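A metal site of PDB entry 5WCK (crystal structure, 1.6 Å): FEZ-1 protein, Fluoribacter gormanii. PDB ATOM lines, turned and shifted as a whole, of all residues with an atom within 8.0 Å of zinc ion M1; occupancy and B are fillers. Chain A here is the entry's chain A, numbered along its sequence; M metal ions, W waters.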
ATOM      1  N   TYR A   2      16.898  11.155  18.466  1.00  0.00           N
ATOM      2  CA  TYR A   2      17.437  12.151  19.409  1.00  0.00           C
ATOM      3  C   TYR A   2      16.646  13.443  19.243  1.00  0.00           C
ATOM      4  O   TYR A   2      16.468  13.924  18.139  1.00  0.00           O
ATOM      5  CB  TYR A   2      18.941  12.383  19.234  1.00  0.00           C
ATOM      6  CG  TYR A   2      19.514  13.068  20.451  1.00  0.00           C
ATOM      7  CD1 TYR A   2      19.812  12.341  21.587  1.00  0.00           C
ATOM      8  CD2 TYR A   2      19.597  14.446  20.527  1.00  0.00           C
ATOM      9  CE1 TYR A   2      20.258  12.959  22.754  1.00  0.00           C
ATOM     10  CE2 TYR A   2      20.036  15.080  21.678  1.00  0.00           C
ATOM     11  CZ  TYR A   2      20.359  14.339  22.801  1.00  0.00           C
ATOM     12  OH  TYR A   2      20.752  14.924  23.972  1.00  0.00           O
ATOM     13  N   ASP A  24      20.933  22.040  24.737  1.00  0.00           N
ATOM     14  CA  ASP A  24      21.150  20.664  25.220  1.00  0.00           C
ATOM     15  C   ASP A  24      22.615  20.282  24.956  1.00  0.00           C
ATOM     16  O   ASP A  24      23.441  20.272  25.880  1.00  0.00           O
ATOM     17  CB  ASP A  24      20.156  19.694  24.580  1.00  0.00           C
ATOM     18  CG  ASP A  24      20.503  18.231  24.805  1.00  0.00           C
ATOM     19  OD1 ASP A  24      21.195  17.942  25.815  1.00  0.00           O
ATOM     20  OD2 ASP A  24      20.105  17.388  23.957  1.00  0.00           O
ATOM     21  N   LEU A  25      22.927  19.969  23.694  1.00  0.00           N
ATOM     22  CA  LEU A  25      24.277  19.584  23.334  1.00  0.00           C
ATOM     23  C   LEU A  25      25.196  20.803  23.494  1.00  0.00           C
ATOM     24  O   LEU A  25      24.911  21.884  22.922  1.00  0.00           O
ATOM     25  CB  LEU A  25      24.273  19.063  21.883  1.00  0.00           C
ATOM     26  CG  LEU A  25      23.264  17.955  21.617  1.00  0.00           C
ATOM     27  CD1 LEU A  25      23.285  17.521  20.153  1.00  0.00           C
ATOM     28  CD2 LEU A  25      23.477  16.781  22.552  1.00  0.00           C
ATOM     29  N   ALA A  26      26.210  20.660  24.357  1.00  0.00           N
ATOM     30  CA  ALA A  26      27.085  21.779  24.780  1.00  0.00           C
ATOM     31  C   ALA A  26      28.371  21.795  23.967  1.00  0.00           C
ATOM     32  O   ALA A  26      29.021  20.770  23.828  1.00  0.00           O
ATOM     33  CB  ALA A  26      27.427  21.640  26.240  1.00  0.00           C
ATOM     34  N   SER A  70      34.055  15.713  23.743  1.00  0.00           N
ATOM     35  CA  SER A  70      33.910  15.102  25.064  1.00  0.00           C
ATOM     36  C   SER A  70      34.025  13.581  24.987  1.00  0.00           C
ATOM     37  O   SER A  70      34.672  12.949  25.800  1.00  0.00           O
ATOM     38  CB  SER A  70      32.588  15.473  25.697  1.00  0.00           C
ATOM     39  OG  SER A  70      32.566  16.855  26.037  1.00  0.00           O
ATOM     40  N   HIS A  71      33.303  12.989  24.038  1.00  0.00           N
ATOM     41  CA  HIS A  71      33.361  11.548  23.858  1.00  0.00           C
ATOM     42  C   HIS A  71      32.753  11.171  22.500  1.00  0.00           C
ATOM     43  O   HIS A  71      32.048  11.965  21.897  1.00  0.00           O
ATOM     44  CB  HIS A  71      32.692  10.803  25.025  1.00  0.00           C
ATOM     45  CG  HIS A  71      31.215  10.955  25.170  1.00  0.00           C
ATOM     46  ND1 HIS A  71      30.633  11.831  26.087  1.00  0.00           N
ATOM     47  CD2 HIS A  71      30.198  10.318  24.564  1.00  0.00           C
ATOM     48  CE1 HIS A  71      29.322  11.697  26.026  1.00  0.00           C
ATOM     49  NE2 HIS A  71      29.018  10.773  25.112  1.00  0.00           N
ATOM     50  N   HIS A  73      30.274   9.726  20.787  1.00  0.00           N
ATOM     51  CA  HIS A  73      28.901   9.426  20.464  1.00  0.00           C
ATOM     52  C   HIS A  73      28.397  10.477  19.458  1.00  0.00           C
ATOM     53  O   HIS A  73      28.866  11.612  19.435  1.00  0.00           O
ATOM     54  CB  HIS A  73      28.006   9.391  21.707  1.00  0.00           C
ATOM     55  CG  HIS A  73      28.098   8.135  22.498  1.00  0.00           C
ATOM     56  ND1 HIS A  73      27.751   8.087  23.864  1.00  0.00           N
ATOM     57  CD2 HIS A  73      28.460   6.881  22.144  1.00  0.00           C
ATOM     58  CE1 HIS A  73      27.903   6.835  24.280  1.00  0.00           C
ATOM     59  NE2 HIS A  73      28.365   6.092  23.274  1.00  0.00           N
ATOM     60  N   PHE A  74      27.411  10.083  18.648  1.00  0.00           N
ATOM     61  CA  PHE A  74      26.919  10.951  17.577  1.00  0.00           C
ATOM     62  C   PHE A  74      26.480  12.329  18.077  1.00  0.00           C
ATOM     63  O   PHE A  74      26.637  13.311  17.336  1.00  0.00           O
ATOM     64  CB  PHE A  74      25.766  10.274  16.810  1.00  0.00           C
ATOM     65  CG  PHE A  74      24.476  10.237  17.577  1.00  0.00           C
ATOM     66  CD1 PHE A  74      24.210   9.227  18.479  1.00  0.00           C
ATOM     67  CD2 PHE A  74      23.534  11.241  17.435  1.00  0.00           C
ATOM     68  CE1 PHE A  74      23.034   9.214  19.225  1.00  0.00           C
ATOM     69  CE2 PHE A  74      22.361  11.237  18.171  1.00  0.00           C
ATOM     70  CZ  PHE A  74      22.112  10.225  19.077  1.00  0.00           C
ATOM     71  N   ASP A  75      25.926  12.416  19.293  1.00  0.00           N
ATOM     72  CA  ASP A  75      25.379  13.684  19.771  1.00  0.00           C
ATOM     73  C   ASP A  75      26.487  14.687  20.095  1.00  0.00           C
ATOM     74  O   ASP A  75      26.178  15.868  20.226  1.00  0.00           O
ATOM     75  CB  ASP A  75      24.420  13.498  20.953  1.00  0.00           C
ATOM     76  CG  ASP A  75      24.968  12.780  22.175  1.00  0.00           C
ATOM     77  OD1 ASP A  75      25.755  11.848  21.977  1.00  0.00           O
ATOM     78  OD2 ASP A  75      24.550  13.116  23.309  1.00  0.00           O
ATOM     79  N   HIS A  76      27.741  14.234  20.245  1.00  0.00           N
ATOM     80  CA  HIS A  76      28.869  15.142  20.486  1.00  0.00           C
ATOM     81  C   HIS A  76      29.815  15.251  19.293  1.00  0.00           C
ATOM     82  O   HIS A  76      30.546  16.252  19.222  1.00  0.00           O
ATOM     83  CB  HIS A  76      29.617  14.723  21.765  1.00  0.00           C
ATOM     84  CG  HIS A  76      28.673  14.586  22.907  1.00  0.00           C
ATOM     85  ND1 HIS A  76      28.058  15.669  23.485  1.00  0.00           N
ATOM     86  CD2 HIS A  76      28.114  13.499  23.473  1.00  0.00           C
ATOM     87  CE1 HIS A  76      27.188  15.246  24.383  1.00  0.00           C
ATOM     88  NE2 HIS A  76      27.222  13.937  24.439  1.00  0.00           N
ATOM     89  N   HIS A 149      31.486   5.551  30.136  1.00  0.00           N
ATOM     90  CA  HIS A 149      30.431   6.005  29.244  1.00  0.00           C
ATOM     91  C   HIS A 149      30.807   5.715  27.785  1.00  0.00           C
ATOM     92  O   HIS A 149      29.966   5.278  26.994  1.00  0.00           O
ATOM     93  CB  HIS A 149      30.074   7.478  29.499  1.00  0.00           C
ATOM     94  CG  HIS A 149      28.975   7.953  28.629  1.00  0.00           C
ATOM     95  ND1 HIS A 149      27.636   7.736  28.927  1.00  0.00           N
ATOM     96  CD2 HIS A 149      29.019   8.578  27.431  1.00  0.00           C
ATOM     97  CE1 HIS A 149      26.900   8.233  27.935  1.00  0.00           C
ATOM     98  NE2 HIS A 149      27.722   8.758  27.011  1.00  0.00           N
ATOM     99  N   GLY A 173      33.033  14.928  30.763  1.00  0.00           N
ATOM    100  CA  GLY A 173      32.728  14.271  29.475  1.00  0.00           C
ATOM    101  C   GLY A 173      31.395  13.540  29.421  1.00  0.00           C
ATOM    102  O   GLY A 173      30.749  13.586  28.375  1.00  0.00           O
ATOM    103  N   SER A 174      31.138  12.839  30.527  1.00  0.00           N
ATOM    104  CA  SER A 174      29.955  12.031  30.967  1.00  0.00           C
ATOM    105  C   SER A 174      30.430  10.822  31.776  1.00  0.00           C
ATOM    106  O   SER A 174      31.299  10.154  31.312  1.00  0.00           O
ATOM    107  CB  SER A 174      29.046  11.460  29.901  1.00  0.00           C
ATOM    108  OG  SER A 174      28.066  10.629  30.463  1.00  0.00           O
ATOM    109  N   ASN A 178      24.235   4.542  30.259  1.00  0.00           N
ATOM    110  CA  ASN A 178      23.100   4.610  29.342  1.00  0.00           C
ATOM    111  C   ASN A 178      22.179   3.413  29.550  1.00  0.00           C
ATOM    112  O   ASN A 178      22.617   2.335  29.916  1.00  0.00           O
ATOM    113  CB  ASN A 178      23.532   4.668  27.887  1.00  0.00           C
ATOM    114  CG  ASN A 178      24.023   6.048  27.488  1.00  0.00           C
ATOM    115  OD1 ASN A 178      23.980   6.997  28.286  1.00  0.00           O
ATOM    116  ND2 ASN A 178      24.463   6.188  26.256  1.00  0.00           N
ATOM    117  N   SER A 214      29.215  17.988  28.864  1.00  0.00           N
ATOM    118  CA  SER A 214      28.856  17.723  27.459  1.00  0.00           C
ATOM    119  C   SER A 214      27.371  18.023  27.175  1.00  0.00           C
ATOM    120  O   SER A 214      27.013  18.227  26.010  1.00  0.00           O
ATOM    121  CB  SER A 214      29.233  16.338  27.104  1.00  0.00           C
ATOM    122  OG  SER A 214      28.645  15.392  27.987  1.00  0.00           O
ATOM    123  N   HIS A 215      26.527  18.035  28.208  1.00  0.00           N
ATOM    124  CA  HIS A 215      25.136  18.391  28.095  1.00  0.00           C
ATOM    125  C   HIS A 215      24.802  19.533  29.075  1.00  0.00           C
ATOM    126  O   HIS A 215      25.215  19.504  30.243  1.00  0.00           O
ATOM    127  CB  HIS A 215      24.196  17.198  28.367  1.00  0.00           C
ATOM    128  CG  HIS A 215      24.233  16.131  27.337  1.00  0.00           C
ATOM    129  ND1 HIS A 215      23.295  16.079  26.325  1.00  0.00           N
ATOM    130  CD2 HIS A 215      25.083  15.103  27.125  1.00  0.00           C
ATOM    131  CE1 HIS A 215      23.551  15.035  25.562  1.00  0.00           C
ATOM    132  NE2 HIS A 215      24.634  14.417  26.023  1.00  0.00           N
ATOM    133  N   MET A 218      23.496  18.885  32.662  1.00  0.00           N
ATOM    134  CA  MET A 218      24.406  18.394  33.704  1.00  0.00           C
ATOM    135  C   MET A 218      24.704  19.515  34.695  1.00  0.00           C
ATOM    136  O   MET A 218      24.885  19.239  35.896  1.00  0.00           O
ATOM    137  CB  MET A 218      25.739  17.917  33.100  1.00  0.00           C
ATOM    138  CG  MET A 218      25.551  16.728  32.248  1.00  0.00           C
ATOM    139  SD  MET A 218      27.111  16.380  31.379  1.00  0.00           S
ATOM    140  CE  MET A 218      26.831  14.699  30.826  1.00  0.00           C
HETATM  141 ZN    ZN M   1      25.508  12.807  25.097  1.00  0.00          ZN
HETATM  142 ZN    ZN M   2      27.284   9.607  25.165  1.00  0.00          ZN
HETATM  143  O   HOH W   1      25.860  10.879  24.651  1.00  0.00           O
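Zinc ion M1 is bound by water W1, the side-chain carboxylate of Asp 75, a ring nitrogen (NE2) of His 215 and a ring nitrogen (NE2) of His 76.
The side-chain sulfur (SD) of Met 218 sits at hydrogen-bond distance from the backbone NH (N) of His 215 (3.6 Å). A ring nitrogen (ND1) of His 215 is in hydrogen-bond range of the side-chain carboxylate (OD1) of Asp 24 (2.9 Å).
Of the 17 residues printed, 3 come within 4 Å of zinc ion M1.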
